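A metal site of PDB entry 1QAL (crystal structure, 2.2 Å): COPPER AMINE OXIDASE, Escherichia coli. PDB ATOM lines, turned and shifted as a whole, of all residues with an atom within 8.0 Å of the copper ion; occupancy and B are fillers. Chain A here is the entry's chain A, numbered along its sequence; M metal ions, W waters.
ND1 of His 519 is in hydrogen-bond range of O of Thr 517 (2.7 Å). A ring nitrogen (ND1) of His 521 lies close to the side-chain hydroxyl (OH) of Tyr 463 (3.2 Å). The backbone carbonyl oxygen of His 521 lies within hydrogen-bond range of the backbone NH of Thr 682, 2.8 Å away. NE2 of His 684 is in hydrogen-bond range of OE1 of Glu 690 (2.6 Å).
A ring nitrogen (NE2) of His 521 binds the copper ion (2.1 Å). NE2 of His 519 is bound to the copper ion. The copper ion is bound by ND1 of His 684 (2.3 Å). Slightly farther from the copper ion lies water W1 (2.6 Å).
Of the 25 residues printed, 3 come within 4 Å of the copper ion.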
ATOM      1  N   VAL A 362      18.212  30.427  -4.638  1.00  0.00           N
ATOM      2  CA  VAL A 362      19.411  29.961  -5.316  1.00  0.00           C
ATOM      3  C   VAL A 362      20.407  31.119  -5.238  1.00  0.00           C
ATOM      4  O   VAL A 362      20.548  31.910  -6.188  1.00  0.00           O
ATOM      5  CB  VAL A 362      19.192  29.506  -6.773  1.00  0.00           C
ATOM      6  CG1 VAL A 362      20.416  28.895  -7.426  1.00  0.00           C
ATOM      7  CG2 VAL A 362      18.012  28.560  -6.840  1.00  0.00           C
ATOM      8  N   TYR A 364      24.144  32.908  -5.080  1.00  0.00           N
ATOM      9  CA  TYR A 364      25.482  32.643  -5.622  1.00  0.00           C
ATOM     10  C   TYR A 364      26.663  33.034  -4.747  1.00  0.00           C
ATOM     11  O   TYR A 364      26.480  33.785  -3.783  1.00  0.00           O
ATOM     12  CB  TYR A 364      25.562  33.237  -7.032  1.00  0.00           C
ATOM     13  CG  TYR A 364      24.839  32.366  -8.037  1.00  0.00           C
ATOM     14  CD1 TYR A 364      23.437  32.341  -8.087  1.00  0.00           C
ATOM     15  CD2 TYR A 364      25.531  31.545  -8.926  1.00  0.00           C
ATOM     16  CE1 TYR A 364      22.765  31.538  -8.997  1.00  0.00           C
ATOM     17  CE2 TYR A 364      24.870  30.750  -9.838  1.00  0.00           C
ATOM     18  CZ  TYR A 364      23.488  30.742  -9.863  1.00  0.00           C
ATOM     19  OH  TYR A 364      22.832  29.942 -10.768  1.00  0.00           O
ATOM     20  N   ASN A 460      16.767  29.929 -16.336  1.00  0.00           N
ATOM     21  CA  ASN A 460      17.546  28.757 -16.679  1.00  0.00           C
ATOM     22  C   ASN A 460      17.286  27.485 -15.872  1.00  0.00           C
ATOM     23  O   ASN A 460      17.719  26.496 -16.432  1.00  0.00           O
ATOM     24  CB  ASN A 460      19.036  29.148 -16.569  1.00  0.00           C
ATOM     25  CG  ASN A 460      19.403  29.744 -15.223  1.00  0.00           C
ATOM     26  OD1 ASN A 460      18.741  30.699 -14.846  1.00  0.00           O
ATOM     27  ND2 ASN A 460      20.422  29.134 -14.632  1.00  0.00           N
ATOM     28  N   TPQ A 461      16.671  27.551 -14.722  1.00  0.00           N
ATOM     29  CA  TPQ A 461      16.525  26.283 -13.997  1.00  0.00           C
ATOM     30  CB  TPQ A 461      16.532  26.467 -12.471  1.00  0.00           C
ATOM     31  C   TPQ A 461      15.202  25.644 -13.989  1.00  0.00           C
ATOM     32  O   TPQ A 461      14.230  26.419 -14.004  1.00  0.00           O
ATOM     33  C1  TPQ A 461      17.589  27.514 -12.045  1.00  0.00           C
ATOM     34  C2  TPQ A 461      18.936  27.168 -11.797  1.00  0.00           C
ATOM     35  O2  TPQ A 461      19.271  26.094 -11.903  1.00  0.00           O
ATOM     36  C3  TPQ A 461      19.897  28.141 -11.409  1.00  0.00           C
ATOM     37  C4  TPQ A 461      19.495  29.456 -11.274  1.00  0.00           C
ATOM     38  O4  TPQ A 461      20.417  30.404 -10.902  1.00  0.00           O
ATOM     39  C5  TPQ A 461      18.185  29.840 -11.508  1.00  0.00           C
ATOM     40  O5  TPQ A 461      17.863  30.909 -11.401  1.00  0.00           O
ATOM     41  C6  TPQ A 461      17.240  28.871 -11.891  1.00  0.00           C
ATOM     42  N   TYR A 463      12.717  23.000 -12.021  1.00  0.00           N
ATOM     43  CA  TYR A 463      12.635  22.322 -10.738  1.00  0.00           C
ATOM     44  C   TYR A 463      11.501  21.300 -10.692  1.00  0.00           C
ATOM     45  O   TYR A 463      10.427  21.701 -11.145  1.00  0.00           O
ATOM     46  CB  TYR A 463      12.479  23.326  -9.606  1.00  0.00           C
ATOM     47  CG  TYR A 463      13.738  24.141  -9.461  1.00  0.00           C
ATOM     48  CD1 TYR A 463      14.914  23.591  -8.931  1.00  0.00           C
ATOM     49  CD2 TYR A 463      13.768  25.466  -9.864  1.00  0.00           C
ATOM     50  CE1 TYR A 463      16.066  24.341  -8.807  1.00  0.00           C
ATOM     51  CE2 TYR A 463      14.894  26.226  -9.742  1.00  0.00           C
ATOM     52  CZ  TYR A 463      16.037  25.669  -9.221  1.00  0.00           C
ATOM     53  OH  TYR A 463      17.128  26.490  -9.132  1.00  0.00           O
ATOM     54  N   ALA A 481      16.593  18.964  -9.602  1.00  0.00           N
ATOM     55  CA  ALA A 481      17.034  20.183 -10.251  1.00  0.00           C
ATOM     56  C   ALA A 481      17.750  19.826 -11.533  1.00  0.00           C
ATOM     57  O   ALA A 481      18.619  18.959 -11.563  1.00  0.00           O
ATOM     58  CB  ALA A 481      18.011  20.965  -9.339  1.00  0.00           C
ATOM     59  N   THR A 482      17.328  20.507 -12.600  1.00  0.00           N
ATOM     60  CA  THR A 482      17.893  20.303 -13.922  1.00  0.00           C
ATOM     61  C   THR A 482      17.836  21.636 -14.653  1.00  0.00           C
ATOM     62  O   THR A 482      17.502  22.714 -14.119  1.00  0.00           O
ATOM     63  CB  THR A 482      17.209  19.163 -14.728  1.00  0.00           C
ATOM     64  OG1 THR A 482      17.811  19.091 -16.044  1.00  0.00           O
ATOM     65  CG2 THR A 482      15.708  19.414 -14.941  1.00  0.00           C
ATOM     66  N   ILE A 484      19.727  24.585 -17.349  1.00  0.00           N
ATOM     67  CA  ILE A 484      20.933  25.214 -17.804  1.00  0.00           C
ATOM     68  C   ILE A 484      21.622  26.018 -16.692  1.00  0.00           C
ATOM     69  O   ILE A 484      21.052  26.893 -16.041  1.00  0.00           O
ATOM     70  CB  ILE A 484      20.590  26.253 -18.922  1.00  0.00           C
ATOM     71  CG1 ILE A 484      19.686  25.689 -20.065  1.00  0.00           C
ATOM     72  CG2 ILE A 484      21.955  26.641 -19.517  1.00  0.00           C
ATOM     73  CD1 ILE A 484      20.120  24.305 -20.584  1.00  0.00           C
ATOM     74  N   GLU A 485      22.906  25.672 -16.527  1.00  0.00           N
ATOM     75  CA  GLU A 485      23.631  26.422 -15.480  1.00  0.00           C
ATOM     76  C   GLU A 485      23.972  27.859 -15.878  1.00  0.00           C
ATOM     77  O   GLU A 485      24.290  28.137 -17.042  1.00  0.00           O
ATOM     78  CB  GLU A 485      24.951  25.718 -15.147  1.00  0.00           C
ATOM     79  CG  GLU A 485      24.748  24.386 -14.410  1.00  0.00           C
ATOM     80  CD  GLU A 485      26.092  23.730 -14.131  1.00  0.00           C
ATOM     81  OE1 GLU A 485      27.006  24.477 -13.709  1.00  0.00           O
ATOM     82  OE2 GLU A 485      26.244  22.506 -14.319  1.00  0.00           O
ATOM     83  N   ALA A 486      23.915  28.774 -14.923  1.00  0.00           N
ATOM     84  CA  ALA A 486      24.251  30.172 -15.031  1.00  0.00           C
ATOM     85  C   ALA A 486      25.795  30.172 -15.074  1.00  0.00           C
ATOM     86  O   ALA A 486      26.422  29.745 -14.083  1.00  0.00           O
ATOM     87  CB  ALA A 486      23.774  30.874 -13.772  1.00  0.00           C
ATOM     88  N   THR A 517      29.583  29.031 -11.975  1.00  0.00           N
ATOM     89  CA  THR A 517      29.728  29.635 -10.672  1.00  0.00           C
ATOM     90  C   THR A 517      29.006  28.887  -9.563  1.00  0.00           C
ATOM     91  O   THR A 517      27.802  28.614  -9.603  1.00  0.00           O
ATOM     92  CB  THR A 517      29.248  31.091 -10.695  1.00  0.00           C
ATOM     93  OG1 THR A 517      29.890  31.780 -11.758  1.00  0.00           O
ATOM     94  CG2 THR A 517      29.391  31.739  -9.332  1.00  0.00           C
ATOM     95  N   THR A 518      29.804  28.594  -8.521  1.00  0.00           N
ATOM     96  CA  THR A 518      29.286  27.888  -7.362  1.00  0.00           C
ATOM     97  C   THR A 518      28.089  28.611  -6.780  1.00  0.00           C
ATOM     98  O   THR A 518      28.064  29.826  -6.819  1.00  0.00           O
ATOM     99  CB  THR A 518      30.377  27.708  -6.274  1.00  0.00           C
ATOM    100  OG1 THR A 518      31.423  26.922  -6.902  1.00  0.00           O
ATOM    101  CG2 THR A 518      29.787  27.027  -5.030  1.00  0.00           C
ATOM    102  N   HIS A 519      27.117  27.857  -6.257  1.00  0.00           N
ATOM    103  CA  HIS A 519      25.933  28.462  -5.651  1.00  0.00           C
ATOM    104  C   HIS A 519      25.216  27.359  -4.875  1.00  0.00           C
ATOM    105  O   HIS A 519      25.699  26.271  -4.886  1.00  0.00           O
ATOM    106  CB  HIS A 519      24.962  28.945  -6.748  1.00  0.00           C
ATOM    107  CG  HIS A 519      24.662  27.821  -7.712  1.00  0.00           C
ATOM    108  ND1 HIS A 519      25.575  27.387  -8.682  1.00  0.00           N
ATOM    109  CD2 HIS A 519      23.541  27.074  -7.813  1.00  0.00           C
ATOM    110  CE1 HIS A 519      25.088  26.397  -9.388  1.00  0.00           C
ATOM    111  NE2 HIS A 519      23.886  26.260  -8.825  1.00  0.00           N
ATOM    112  N   GLN A 520      24.112  27.659  -4.211  1.00  0.00           N
ATOM    113  CA  GLN A 520      23.364  26.640  -3.497  1.00  0.00           C
ATOM    114  C   GLN A 520      21.919  26.627  -4.032  1.00  0.00           C
ATOM    115  O   GLN A 520      21.412  27.585  -4.618  1.00  0.00           O
ATOM    116  CB  GLN A 520      23.240  27.132  -2.045  1.00  0.00           C
ATOM    117  CG  GLN A 520      24.612  27.084  -1.356  1.00  0.00           C
ATOM    118  CD  GLN A 520      24.475  27.303   0.130  1.00  0.00           C
ATOM    119  OE1 GLN A 520      24.370  26.257   0.779  1.00  0.00           O
ATOM    120  NE2 GLN A 520      24.481  28.561   0.537  1.00  0.00           N
ATOM    121  N   HIS A 521      21.235  25.533  -3.771  1.00  0.00           N
ATOM    122  CA  HIS A 521      19.827  25.320  -4.131  1.00  0.00           C
ATOM    123  C   HIS A 521      19.242  25.049  -2.723  1.00  0.00           C
ATOM    124  O   HIS A 521      19.587  24.060  -2.082  1.00  0.00           O
ATOM    125  CB  HIS A 521      19.629  24.087  -5.004  1.00  0.00           C
ATOM    126  CG  HIS A 521      20.096  24.314  -6.397  1.00  0.00           C
ATOM    127  ND1 HIS A 521      19.318  25.026  -7.307  1.00  0.00           N
ATOM    128  CD2 HIS A 521      21.222  23.959  -7.029  1.00  0.00           C
ATOM    129  CE1 HIS A 521      19.925  25.109  -8.477  1.00  0.00           C
ATOM    130  NE2 HIS A 521      21.043  24.467  -8.280  1.00  0.00           N
ATOM    131  N   TYR A 523      15.674  24.592  -0.655  1.00  0.00           N
ATOM    132  CA  TYR A 523      14.220  24.498  -0.686  1.00  0.00           C
ATOM    133  C   TYR A 523      13.719  24.482   0.750  1.00  0.00           C
ATOM    134  O   TYR A 523      14.375  23.956   1.652  1.00  0.00           O
ATOM    135  CB  TYR A 523      13.726  23.185  -1.382  1.00  0.00           C
ATOM    136  CG  TYR A 523      14.507  22.847  -2.629  1.00  0.00           C
ATOM    137  CD1 TYR A 523      14.036  23.397  -3.834  1.00  0.00           C
ATOM    138  CD2 TYR A 523      15.622  22.056  -2.673  1.00  0.00           C
ATOM    139  CE1 TYR A 523      14.681  23.147  -5.034  1.00  0.00           C
ATOM    140  CE2 TYR A 523      16.266  21.805  -3.873  1.00  0.00           C
ATOM    141  CZ  TYR A 523      15.790  22.351  -5.035  1.00  0.00           C
ATOM    142  OH  TYR A 523      16.435  22.101  -6.234  1.00  0.00           O
ATOM    143  N   HIS A 608      23.843  15.624  -4.884  1.00  0.00           N
ATOM    144  CA  HIS A 608      24.789  16.727  -4.934  1.00  0.00           C
ATOM    145  C   HIS A 608      25.255  16.958  -3.486  1.00  0.00           C
ATOM    146  O   HIS A 608      24.601  16.522  -2.553  1.00  0.00           O
ATOM    147  CB  HIS A 608      24.124  17.993  -5.434  1.00  0.00           C
ATOM    148  CG  HIS A 608      24.455  18.412  -6.836  1.00  0.00           C
ATOM    149  ND1 HIS A 608      23.807  19.445  -7.480  1.00  0.00           N
ATOM    150  CD2 HIS A 608      25.376  17.905  -7.692  1.00  0.00           C
ATOM    151  CE1 HIS A 608      24.314  19.574  -8.701  1.00  0.00           C
ATOM    152  NE2 HIS A 608      25.260  18.650  -8.826  1.00  0.00           N
ATOM    153  N   THR A 682      21.453  22.169  -1.278  1.00  0.00           N
ATOM    154  CA  THR A 682      22.658  21.535  -1.806  1.00  0.00           C
ATOM    155  C   THR A 682      23.619  22.682  -2.135  1.00  0.00           C
ATOM    156  O   THR A 682      23.213  23.822  -2.372  1.00  0.00           O
ATOM    157  CB  THR A 682      22.361  20.846  -3.154  1.00  0.00           C
ATOM    158  OG1 THR A 682      22.252  21.929  -4.117  1.00  0.00           O
ATOM    159  CG2 THR A 682      21.126  19.947  -3.148  1.00  0.00           C
ATOM    160  N   THR A 683      24.900  22.365  -2.174  1.00  0.00           N
ATOM    161  CA  THR A 683      25.917  23.325  -2.517  1.00  0.00           C
ATOM    162  C   THR A 683      26.359  22.747  -3.878  1.00  0.00           C
ATOM    163  O   THR A 683      26.852  21.605  -3.906  1.00  0.00           O
ATOM    164  CB  THR A 683      27.092  23.316  -1.528  1.00  0.00           C
ATOM    165  OG1 THR A 683      26.615  23.996  -0.383  1.00  0.00           O
ATOM    166  CG2 THR A 683      28.212  24.161  -2.125  1.00  0.00           C
ATOM    167  N   HIS A 684      26.166  23.585  -4.920  1.00  0.00           N
ATOM    168  CA  HIS A 684      26.558  23.045  -6.218  1.00  0.00           C
ATOM    169  C   HIS A 684      27.872  23.525  -6.769  1.00  0.00           C
ATOM    170  O   HIS A 684      28.028  24.690  -7.147  1.00  0.00           O
ATOM    171  CB  HIS A 684      25.411  23.371  -7.222  1.00  0.00           C
ATOM    172  CG  HIS A 684      25.619  22.815  -8.594  1.00  0.00           C
ATOM    173  ND1 HIS A 684      24.777  23.017  -9.653  1.00  0.00           N
ATOM    174  CD2 HIS A 684      26.567  22.048  -9.153  1.00  0.00           C
ATOM    175  CE1 HIS A 684      25.148  22.441 -10.763  1.00  0.00           C
ATOM    176  NE2 HIS A 684      26.274  21.815 -10.474  1.00  0.00           N
ATOM    177  N   VAL A 685      28.840  22.644  -6.852  1.00  0.00           N
ATOM    178  CA  VAL A 685      30.171  22.935  -7.404  1.00  0.00           C
ATOM    179  C   VAL A 685      30.082  22.126  -8.704  1.00  0.00           C
ATOM    180  O   VAL A 685      30.113  20.897  -8.720  1.00  0.00           O
ATOM    181  CB  VAL A 685      31.327  22.417  -6.524  1.00  0.00           C
ATOM    182  CG1 VAL A 685      32.744  22.435  -7.128  1.00  0.00           C
ATOM    183  CG2 VAL A 685      31.396  23.214  -5.232  1.00  0.00           C
ATOM    184  N   ALA A 686      29.984  22.763  -9.840  1.00  0.00           N
ATOM    185  CA  ALA A 686      29.853  22.225 -11.178  1.00  0.00           C
ATOM    186  C   ALA A 686      30.950  21.324 -11.682  1.00  0.00           C
ATOM    187  O   ALA A 686      32.026  21.226 -11.079  1.00  0.00           O
ATOM    188  CB  ALA A 686      29.602  23.366 -12.181  1.00  0.00           C
ATOM    189  N   GLU A 690      27.813  18.408 -16.546  1.00  0.00           N
ATOM    190  CA  GLU A 690      26.569  19.161 -16.405  1.00  0.00           C
ATOM    191  C   GLU A 690      26.375  20.268 -17.431  1.00  0.00           C
ATOM    192  O   GLU A 690      25.518  21.165 -17.319  1.00  0.00           O
ATOM    193  CB  GLU A 690      26.531  19.734 -14.976  1.00  0.00           C
ATOM    194  CG  GLU A 690      26.894  18.742 -13.852  1.00  0.00           C
ATOM    195  CD  GLU A 690      27.045  19.466 -12.515  1.00  0.00           C
ATOM    196  OE1 GLU A 690      27.547  20.601 -12.358  1.00  0.00           O
ATOM    197  OE2 GLU A 690      26.633  18.908 -11.474  1.00  0.00           O
ATOM    198  N   MET A 694      22.278  20.128 -17.551  1.00  0.00           N
ATOM    199  CA  MET A 694      22.519  19.344 -16.351  1.00  0.00           C
ATOM    200  C   MET A 694      21.617  18.168 -16.057  1.00  0.00           C
ATOM    201  O   MET A 694      20.425  18.362 -15.913  1.00  0.00           O
ATOM    202  CB  MET A 694      22.450  20.216 -15.063  1.00  0.00           C
ATOM    203  CG  MET A 694      22.947  19.493 -13.797  1.00  0.00           C
ATOM    204  SD  MET A 694      22.958  20.528 -12.284  1.00  0.00           S
ATOM    205  CE  MET A 694      21.282  20.197 -11.719  1.00  0.00           C
ATOM    206  N   GLU A 697      19.465  16.358 -10.682  1.00  0.00           N
ATOM    207  CA  GLU A 697      20.032  16.029  -9.381  1.00  0.00           C
ATOM    208  C   GLU A 697      18.877  16.055  -8.372  1.00  0.00           C
ATOM    209  O   GLU A 697      18.002  16.946  -8.449  1.00  0.00           O
ATOM    210  CB  GLU A 697      21.102  17.022  -8.917  1.00  0.00           C
ATOM    211  CG  GLU A 697      22.294  17.065  -9.849  1.00  0.00           C
ATOM    212  CD  GLU A 697      23.295  15.981  -9.613  1.00  0.00           C
ATOM    213  OE1 GLU A 697      23.002  15.119  -8.743  1.00  0.00           O
ATOM    214  OE2 GLU A 697      24.330  16.039 -10.306  1.00  0.00           O
HETATM  215 CU    CU M   1      22.863  24.348  -9.402  1.00  0.00          CU
HETATM  216  O   HOH W   1      21.937  25.476 -11.564  1.00  0.00           O
